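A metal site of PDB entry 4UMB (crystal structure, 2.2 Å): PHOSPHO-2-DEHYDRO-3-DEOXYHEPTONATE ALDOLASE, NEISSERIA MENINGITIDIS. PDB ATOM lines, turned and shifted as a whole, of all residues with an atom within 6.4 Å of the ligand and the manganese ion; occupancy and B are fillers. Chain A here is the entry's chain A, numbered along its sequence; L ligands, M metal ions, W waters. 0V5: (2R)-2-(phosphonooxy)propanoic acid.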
ATOM      1  N   PRO A  62     -17.579 -27.230  -8.676  1.00  0.00           N
ATOM      2  CA  PRO A  62     -16.585 -26.223  -8.994  1.00  0.00           C
ATOM      3  C   PRO A  62     -16.299 -25.252  -7.868  1.00  0.00           C
ATOM      4  O   PRO A  62     -17.194 -24.942  -7.062  1.00  0.00           O
ATOM      5  CB  PRO A  62     -17.255 -25.466 -10.140  1.00  0.00           C
ATOM      6  CG  PRO A  62     -18.081 -26.508 -10.837  1.00  0.00           C
ATOM      7  CD  PRO A  62     -18.630 -27.319  -9.703  1.00  0.00           C
ATOM      8  N   CYS A  63     -15.082 -24.725  -7.852  1.00  0.00           N
ATOM      9  CA  CYS A  63     -14.788 -23.614  -6.966  1.00  0.00           C
ATOM     10  C   CYS A  63     -15.787 -22.477  -7.220  1.00  0.00           C
ATOM     11  O   CYS A  63     -16.373 -21.910  -6.282  1.00  0.00           O
ATOM     12  CB  CYS A  63     -13.351 -23.115  -7.146  1.00  0.00           C
ATOM     13  SG  CYS A  63     -13.003 -21.624  -6.174  1.00  0.00           S
ATOM     14  N   SER A  64     -15.991 -22.173  -8.505  1.00  0.00           N
ATOM     15  CA  SER A  64     -16.922 -21.124  -8.933  1.00  0.00           C
ATOM     16  C   SER A  64     -17.623 -21.516 -10.207  1.00  0.00           C
ATOM     17  O   SER A  64     -17.045 -22.217 -11.053  1.00  0.00           O
ATOM     18  CB  SER A  64     -16.172 -19.832  -9.174  1.00  0.00           C
ATOM     19  OG  SER A  64     -15.146 -20.015 -10.148  1.00  0.00           O
ATOM     20  N   ARG A  94     -21.784 -27.915  -5.468  1.00  0.00           N
ATOM     21  CA  ARG A  94     -21.267 -26.534  -5.302  1.00  0.00           C
ATOM     22  C   ARG A  94     -21.670 -25.679  -6.479  1.00  0.00           C
ATOM     23  O   ARG A  94     -21.298 -25.996  -7.641  1.00  0.00           O
ATOM     24  CB  ARG A  94     -19.728 -26.513  -5.237  1.00  0.00           C
ATOM     25  CG  ARG A  94     -19.100 -27.035  -3.942  1.00  0.00           C
ATOM     26  CD  ARG A  94     -17.570 -26.958  -3.954  1.00  0.00           C
ATOM     27  NE  ARG A  94     -17.071 -25.622  -4.247  1.00  0.00           N
ATOM     28  CZ  ARG A  94     -16.539 -24.767  -3.362  1.00  0.00           C
ATOM     29  NH1 ARG A  94     -16.319 -25.108  -2.098  1.00  0.00           N
ATOM     30  NH2 ARG A  94     -16.192 -23.541  -3.757  1.00  0.00           N
ATOM     31  N   TYR A  96     -21.429 -22.010  -6.616  1.00  0.00           N
ATOM     32  CA  TYR A  96     -20.972 -20.769  -6.006  1.00  0.00           C
ATOM     33  C   TYR A  96     -20.978 -19.588  -6.990  1.00  0.00           C
ATOM     34  O   TYR A  96     -20.294 -19.610  -8.021  1.00  0.00           O
ATOM     35  CB  TYR A  96     -19.551 -20.975  -5.447  1.00  0.00           C
ATOM     36  CG  TYR A  96     -19.481 -21.678  -4.100  1.00  0.00           C
ATOM     37  CD1 TYR A  96     -20.168 -22.866  -3.848  1.00  0.00           C
ATOM     38  CD2 TYR A  96     -18.655 -21.174  -3.081  1.00  0.00           C
ATOM     39  CE1 TYR A  96     -20.066 -23.512  -2.621  1.00  0.00           C
ATOM     40  CE2 TYR A  96     -18.544 -21.814  -1.846  1.00  0.00           C
ATOM     41  CZ  TYR A  96     -19.238 -22.961  -1.623  1.00  0.00           C
ATOM     42  OH  TYR A  96     -19.132 -23.574  -0.419  1.00  0.00           O
ATOM     43  N   GLU A  98     -20.570 -16.249  -5.767  1.00  0.00           N
ATOM     44  CA  GLU A  98     -19.933 -15.113  -5.086  1.00  0.00           C
ATOM     45  C   GLU A  98     -18.594 -15.546  -4.479  1.00  0.00           C
ATOM     46  O   GLU A  98     -18.541 -16.467  -3.680  1.00  0.00           O
ATOM     47  CB  GLU A  98     -20.868 -14.593  -3.991  1.00  0.00           C
ATOM     48  CG  GLU A  98     -22.215 -14.117  -4.518  1.00  0.00           C
ATOM     49  CD  GLU A  98     -23.238 -13.785  -3.439  1.00  0.00           C
ATOM     50  OE1 GLU A  98     -22.924 -13.851  -2.230  1.00  0.00           O
ATOM     51  OE2 GLU A  98     -24.372 -13.437  -3.814  1.00  0.00           O
ATOM     52  N   LYS A  99     -17.514 -14.907  -4.900  1.00  0.00           N
ATOM     53  CA  LYS A  99     -16.170 -15.296  -4.494  1.00  0.00           C
ATOM     54  C   LYS A  99     -15.473 -14.165  -3.729  1.00  0.00           C
ATOM     55  O   LYS A  99     -15.391 -13.043  -4.209  1.00  0.00           O
ATOM     56  CB  LYS A  99     -15.333 -15.661  -5.696  1.00  0.00           C
ATOM     57  CG  LYS A  99     -15.939 -16.734  -6.575  1.00  0.00           C
ATOM     58  CD  LYS A  99     -16.311 -18.007  -5.821  1.00  0.00           C
ATOM     59  CE  LYS A  99     -15.097 -18.708  -5.266  1.00  0.00           C
ATOM     60  NZ  LYS A  99     -15.483 -19.906  -4.456  1.00  0.00           N
ATOM     61  N   PRO A 100     -14.984 -14.468  -2.528  1.00  0.00           N
ATOM     62  CA  PRO A 100     -14.241 -13.483  -1.754  1.00  0.00           C
ATOM     63  C   PRO A 100     -12.792 -13.554  -2.163  1.00  0.00           C
ATOM     64  O   PRO A 100     -12.192 -14.607  -2.081  1.00  0.00           O
ATOM     65  CB  PRO A 100     -14.448 -13.940  -0.307  1.00  0.00           C
ATOM     66  CG  PRO A 100     -14.559 -15.443  -0.411  1.00  0.00           C
ATOM     67  CD  PRO A 100     -15.155 -15.734  -1.778  1.00  0.00           C
ATOM     68  N   GLU A 145     -21.771 -20.178  -1.304  1.00  0.00           N
ATOM     69  CA  GLU A 145     -21.360 -19.279  -0.221  1.00  0.00           C
ATOM     70  C   GLU A 145     -22.243 -18.064  -0.305  1.00  0.00           C
ATOM     71  O   GLU A 145     -22.366 -17.422  -1.360  1.00  0.00           O
ATOM     72  CB  GLU A 145     -19.869 -18.861  -0.302  1.00  0.00           C
ATOM     73  CG  GLU A 145     -19.530 -17.723   0.681  1.00  0.00           C
ATOM     74  CD  GLU A 145     -18.069 -17.316   0.750  1.00  0.00           C
ATOM     75  OE1 GLU A 145     -17.203 -18.053   0.186  1.00  0.00           O
ATOM     76  OE2 GLU A 145     -17.800 -16.277   1.364  1.00  0.00           O
ATOM     77  N   ILE A 164     -20.839 -19.872   5.028  1.00  0.00           N
ATOM     78  CA  ILE A 164     -20.237 -18.579   5.328  1.00  0.00           C
ATOM     79  C   ILE A 164     -18.734 -18.808   5.327  1.00  0.00           C
ATOM     80  O   ILE A 164     -18.228 -19.650   6.045  1.00  0.00           O
ATOM     81  CB  ILE A 164     -20.685 -18.006   6.694  1.00  0.00           C
ATOM     82  CG1 ILE A 164     -22.205 -17.850   6.718  1.00  0.00           C
ATOM     83  CG2 ILE A 164     -19.984 -16.696   6.996  1.00  0.00           C
ATOM     84  CD1 ILE A 164     -22.786 -16.862   5.719  1.00  0.00           C
ATOM     85  N   GLY A 165     -18.019 -18.037   4.536  1.00  0.00           N
ATOM     86  CA  GLY A 165     -16.621 -18.296   4.274  1.00  0.00           C
ATOM     87  C   GLY A 165     -15.694 -18.030   5.457  1.00  0.00           C
ATOM     88  O   GLY A 165     -16.030 -17.326   6.406  1.00  0.00           O
ATOM     89  N   ALA A 166     -14.482 -18.569   5.351  1.00  0.00           N
ATOM     90  CA  ALA A 166     -13.453 -18.355   6.350  1.00  0.00           C
ATOM     91  C   ALA A 166     -13.220 -16.862   6.636  1.00  0.00           C
ATOM     92  O   ALA A 166     -12.900 -16.490   7.764  1.00  0.00           O
ATOM     93  CB  ALA A 166     -12.155 -19.013   5.899  1.00  0.00           C
ATOM     94  N   ARG A 167     -13.355 -16.037   5.599  1.00  0.00           N
ATOM     95  CA  ARG A 167     -13.038 -14.605   5.693  1.00  0.00           C
ATOM     96  C   ARG A 167     -14.150 -13.741   6.284  1.00  0.00           C
ATOM     97  O   ARG A 167     -13.932 -12.569   6.593  1.00  0.00           O
ATOM     98  CB  ARG A 167     -12.644 -14.060   4.308  1.00  0.00           C
ATOM     99  CG  ARG A 167     -11.327 -14.647   3.796  1.00  0.00           C
ATOM    100  CD  ARG A 167     -11.041 -14.290   2.331  1.00  0.00           C
ATOM    101  NE  ARG A 167      -9.964 -15.133   1.794  1.00  0.00           N
ATOM    102  CZ  ARG A 167     -10.088 -16.434   1.525  1.00  0.00           C
ATOM    103  NH1 ARG A 167     -11.223 -17.092   1.671  1.00  0.00           N
ATOM    104  NH2 ARG A 167      -9.012 -17.105   1.126  1.00  0.00           N
ATOM    105  N   LYS A 188     -17.090 -21.631   8.338  1.00  0.00           N
ATOM    106  CA  LYS A 188     -15.720 -22.083   8.229  1.00  0.00           C
ATOM    107  C   LYS A 188     -14.827 -21.445   9.298  1.00  0.00           C
ATOM    108  O   LYS A 188     -15.032 -20.298   9.691  1.00  0.00           O
ATOM    109  CB  LYS A 188     -15.195 -21.755   6.839  1.00  0.00           C
ATOM    110  CG  LYS A 188     -15.945 -22.513   5.724  1.00  0.00           C
ATOM    111  CD  LYS A 188     -15.256 -22.375   4.377  1.00  0.00           C
ATOM    112  CE  LYS A 188     -15.308 -23.653   3.565  1.00  0.00           C
ATOM    113  NZ  LYS A 188     -14.333 -23.593   2.441  1.00  0.00           N
ATOM    114  N   ASN A 189     -13.842 -22.220   9.752  1.00  0.00           N
ATOM    115  CA  ASN A 189     -12.790 -21.664  10.581  1.00  0.00           C
ATOM    116  C   ASN A 189     -12.073 -20.559   9.805  1.00  0.00           C
ATOM    117  O   ASN A 189     -12.142 -20.502   8.560  1.00  0.00           O
ATOM    118  CB  ASN A 189     -11.829 -22.768  11.099  1.00  0.00           C
ATOM    119  CG  ASN A 189     -10.997 -23.459   9.998  1.00  0.00           C
ATOM    120  OD1 ASN A 189     -11.191 -24.654   9.721  1.00  0.00           O
ATOM    121  ND2 ASN A 189     -10.009 -22.755   9.447  1.00  0.00           N
ATOM    122  N   THR A 191      -8.994 -18.058   8.254  1.00  0.00           N
ATOM    123  CA  THR A 191      -7.948 -18.415   7.293  1.00  0.00           C
ATOM    124  C   THR A 191      -6.627 -18.805   7.965  1.00  0.00           C
ATOM    125  O   THR A 191      -5.832 -19.541   7.366  1.00  0.00           O
ATOM    126  CB  THR A 191      -7.738 -17.299   6.235  1.00  0.00           C
ATOM    127  OG1 THR A 191      -7.494 -16.063   6.906  1.00  0.00           O
ATOM    128  CG2 THR A 191      -8.951 -17.163   5.372  1.00  0.00           C
ATOM    129  N   ARG A 236     -11.492 -26.281   7.395  1.00  0.00           N
ATOM    130  CA  ARG A 236     -10.954 -26.032   6.049  1.00  0.00           C
ATOM    131  C   ARG A 236      -9.478 -25.652   6.077  1.00  0.00           C
ATOM    132  O   ARG A 236      -8.947 -25.099   5.107  1.00  0.00           O
ATOM    133  CB  ARG A 236     -11.786 -24.959   5.300  1.00  0.00           C
ATOM    134  CG  ARG A 236     -12.036 -23.689   6.103  1.00  0.00           C
ATOM    135  CD  ARG A 236     -10.838 -22.768   6.138  1.00  0.00           C
ATOM    136  NE  ARG A 236     -10.632 -22.134   4.838  1.00  0.00           N
ATOM    137  CZ  ARG A 236      -9.520 -21.510   4.493  1.00  0.00           C
ATOM    138  NH1 ARG A 236      -8.478 -21.475   5.324  1.00  0.00           N
ATOM    139  NH2 ARG A 236      -9.440 -20.921   3.316  1.00  0.00           N
ATOM    140  N   ASP A 267     -13.511 -29.800   4.889  1.00  0.00           N
ATOM    141  CA  ASP A 267     -13.225 -29.389   3.534  1.00  0.00           C
ATOM    142  C   ASP A 267     -11.921 -30.083   3.119  1.00  0.00           C
ATOM    143  O   ASP A 267     -10.898 -29.931   3.770  1.00  0.00           O
ATOM    144  CB  ASP A 267     -13.107 -27.858   3.484  1.00  0.00           C
ATOM    145  CG  ASP A 267     -12.888 -27.297   2.077  1.00  0.00           C
ATOM    146  OD1 ASP A 267     -12.764 -28.061   1.093  1.00  0.00           O
ATOM    147  OD2 ASP A 267     -12.851 -26.053   1.971  1.00  0.00           O
ATOM    148  N   SER A 269     -10.386 -29.311   0.371  1.00  0.00           N
ATOM    149  CA  SER A 269      -9.653 -28.351  -0.439  1.00  0.00           C
ATOM    150  C   SER A 269      -9.109 -27.160   0.412  1.00  0.00           C
ATOM    151  O   SER A 269      -8.893 -27.297   1.633  1.00  0.00           O
ATOM    152  CB  SER A 269     -10.552 -27.851  -1.596  1.00  0.00           C
ATOM    153  OG  SER A 269      -9.786 -27.353  -2.681  1.00  0.00           O
ATOM    154  N   HIS A 270      -8.818 -26.060  -0.270  1.00  0.00           N
ATOM    155  CA  HIS A 270      -8.282 -24.868   0.323  1.00  0.00           C
ATOM    156  C   HIS A 270      -7.085 -25.195   1.216  1.00  0.00           C
ATOM    157  O   HIS A 270      -6.140 -25.809   0.737  1.00  0.00           O
ATOM    158  CB  HIS A 270      -9.427 -24.105   0.955  1.00  0.00           C
ATOM    159  CG  HIS A 270     -10.540 -23.897  -0.005  1.00  0.00           C
ATOM    160  ND1 HIS A 270     -11.712 -24.631   0.042  1.00  0.00           N
ATOM    161  CD2 HIS A 270     -10.623 -23.135  -1.126  1.00  0.00           C
ATOM    162  CE1 HIS A 270     -12.481 -24.299  -0.982  1.00  0.00           C
ATOM    163  NE2 HIS A 270     -11.841 -23.393  -1.705  1.00  0.00           N
ATOM    164  N   ALA A 271      -7.097 -24.790   2.487  1.00  0.00           N
ATOM    165  CA  ALA A 271      -5.887 -24.906   3.310  1.00  0.00           C
ATOM    166  C   ALA A 271      -5.674 -26.319   3.797  1.00  0.00           C
ATOM    167  O   ALA A 271      -4.596 -26.643   4.270  1.00  0.00           O
ATOM    168  CB  ALA A 271      -5.927 -23.934   4.479  1.00  0.00           C
ATOM    169  N   MET A 302     -16.423 -31.499   1.968  1.00  0.00           N
ATOM    170  CA  MET A 302     -16.497 -30.557   0.871  1.00  0.00           C
ATOM    171  C   MET A 302     -15.363 -30.890  -0.095  1.00  0.00           C
ATOM    172  O   MET A 302     -14.281 -31.293   0.335  1.00  0.00           O
ATOM    173  CB  MET A 302     -16.407 -29.135   1.406  1.00  0.00           C
ATOM    174  CG  MET A 302     -16.573 -28.018   0.384  1.00  0.00           C
ATOM    175  SD  MET A 302     -16.708 -26.365   1.158  1.00  0.00           S
ATOM    176  CE  MET A 302     -17.155 -26.859   2.819  1.00  0.00           C
ATOM    177  N   GLU A 304     -13.641 -29.665  -4.132  1.00  0.00           N
ATOM    178  CA  GLU A 304     -13.591 -28.847  -5.310  1.00  0.00           C
ATOM    179  C   GLU A 304     -13.284 -29.714  -6.553  1.00  0.00           C
ATOM    180  O   GLU A 304     -12.159 -30.158  -6.749  1.00  0.00           O
ATOM    181  CB  GLU A 304     -12.574 -27.707  -5.132  1.00  0.00           C
ATOM    182  CG  GLU A 304     -13.094 -26.648  -4.145  1.00  0.00           C
ATOM    183  CD  GLU A 304     -12.317 -25.354  -4.129  1.00  0.00           C
ATOM    184  OE1 GLU A 304     -11.079 -25.351  -4.018  1.00  0.00           O
ATOM    185  OE2 GLU A 304     -12.995 -24.317  -4.198  1.00  0.00           O
ATOM    186  N   THR A 323     -11.036 -20.129 -11.023  1.00  0.00           N
ATOM    187  CA  THR A 323     -10.642 -19.729  -9.647  1.00  0.00           C
ATOM    188  C   THR A 323      -9.741 -20.845  -9.080  1.00  0.00           C
ATOM    189  O   THR A 323      -8.756 -21.215  -9.747  1.00  0.00           O
ATOM    190  CB  THR A 323     -11.871 -19.370  -8.797  1.00  0.00           C
ATOM    191  OG1 THR A 323     -12.893 -20.367  -8.929  1.00  0.00           O
ATOM    192  CG2 THR A 323     -12.457 -18.028  -9.260  1.00  0.00           C
ATOM    193  N   ASP A 324     -10.051 -21.396  -7.899  1.00  0.00           N
ATOM    194  CA  ASP A 324      -9.157 -22.412  -7.328  1.00  0.00           C
ATOM    195  C   ASP A 324      -9.128 -23.626  -8.259  1.00  0.00           C
ATOM    196  O   ASP A 324     -10.130 -23.962  -8.879  1.00  0.00           O
ATOM    197  CB  ASP A 324      -9.613 -22.900  -5.953  1.00  0.00           C
ATOM    198  CG  ASP A 324      -9.695 -21.795  -4.917  1.00  0.00           C
ATOM    199  OD1 ASP A 324      -8.918 -20.833  -5.038  1.00  0.00           O
ATOM    200  OD2 ASP A 324     -10.537 -21.904  -3.999  1.00  0.00           O
HETATM  201  C1  0V5 L   1     -14.151 -21.572  -1.696  1.00  0.00           C
HETATM  202  O1  0V5 L   1     -13.752 -21.408  -2.867  1.00  0.00           O
HETATM  203  O2' 0V5 L   1     -15.042 -22.359  -1.319  1.00  0.00           O
HETATM  204  C2  0V5 L   1     -13.486 -20.677  -0.662  1.00  0.00           C
HETATM  205  C3  0V5 L   1     -14.112 -19.295  -0.852  1.00  0.00           C
HETATM  206  O2  0V5 L   1     -13.709 -21.153   0.673  1.00  0.00           O
HETATM  207  P   0V5 L   1     -12.798 -20.568   1.891  1.00  0.00           P
HETATM  208  O1P 0V5 L   1     -13.819 -19.592   2.637  1.00  0.00           O
HETATM  209  O2P 0V5 L   1     -12.575 -21.778   2.924  1.00  0.00           O
HETATM  210  O3P 0V5 L   1     -11.601 -19.783   1.422  1.00  0.00           O
HETATM  211 MN    MN M   1     -12.291 -22.453  -3.814  1.00  0.00          MN
HETATM  212  O   HOH W   1     -16.931 -18.478  -2.465  1.00  0.00           O
HETATM  213  O   HOH W   2     -16.806 -22.715   0.709  1.00  0.00           O
HETATM  214  O   HOH W   3     -13.727 -16.827   2.761  1.00  0.00           O
HETATM  215  O   HOH W   4     -16.416 -20.249   1.701  1.00  0.00           O
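The side-chain amino group of Lys 188 is in salt-bridge range of an oxygen (O2P) of the ligand, at 2.6 Å. NH2 of Arg 94 lies within salt-bridge range of O2' of the ligand, 2.9 Å away. An oxygen (O2P) of the ligand is in salt-bridge range of the guanidinium group of Arg 236 (2.8 Å). NH1 of Arg 167 is in salt-bridge range of O3P of the ligand, at 2.7 Å. The backbone NH of Ala 166 lies within hydrogen-bond range of an oxygen (O1P) of the ligand (3.0 Å). An oxygen (O1) of the ligand sits close to the side-chain amino group (NZ) of Lys 99 (2.8 Å).
The guanidinium group (NE) of Arg 94 sits at hydrogen-bond distance from the backbone carbonyl oxygen (O) of Pro 62, at 2.9 Å. The side-chain sulfur of Met 302 sits at hydrogen-bond distance from the guanidinium group of Arg 94, at 3.5 Å. The side-chain amino group (NZ) of Lys 99 lies within hydrogen-bond range of the backbone carbonyl oxygen (O) of Cys 63 (2.9 Å). The side-chain carboxylate of Glu 304 lies close to the guanidinium group of Arg 94 (3.3 Å). O of Cys 63 sits at hydrogen-bond distance from NH2 of Arg 94 (3.0 Å). The side-chain hydroxyl (OG) of Ser 269 lies within hydrogen-bond range of the side-chain carboxylate (OE1) of Glu 304 (2.7 Å). N of Arg 236 lies within hydrogen-bond range of OD1 of Asn 189, at 2.9 Å. O of Arg 236 sits at hydrogen-bond distance from N of Ala 271.
Residues that only touch the ligand: Tyr 96 (3.6 Å), Pro 100 (3.8 Å), Glu 145 (3.5 Å) and Gly 165 (3.5 Å). Hydrophobic or aromatic side chains within 4 Å of the ligand: Tyr 96, Pro 100, Ala 166 and His 270. Of the 25 residues printed, 14 come within 4 Å of the ligand.
Within 4 Å of the manganese ion: Cys 63, His 270, Glu 304 and Asp 324.
The manganese ion is bound by OD2 of Asp 324 (1.8 Å), OE2 of Glu 304 (2.0 Å), O1 of the ligand (2.0 Å), NE2 of His 270 (2.4 Å) and SG of Cys 63 (2.6 Å). The manganese ion has five donor atoms within binding distance.
Water W2 lies within hydrogen-bond range of an oxygen (O2') of the ligand (2.7 Å), the side-chain hydroxyl (OH) of Tyr 96 (2.7 Å), the side-chain amino group (NZ) of Lys 188 (3.1 Å) and the side-chain sulfur (SD) of Met 302 (3.7 Å). Water W3 lies within hydrogen-bond range of the guanidinium group (NH1) of Arg 167 (2.7 Å), an oxygen (O1P) of the ligand (2.8 Å) and the backbone NH (N) of Ala 166 (3.2 Å). Water W4 lies within hydrogen-bond range of the side-chain carboxylate of Glu 145 (2.8 Å) and an oxygen (O1P) of the ligand (2.8 Å). Water W1 lies within hydrogen-bond range of OE1 of Glu 145, NZ of Lys 99 and O of Glu 98.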
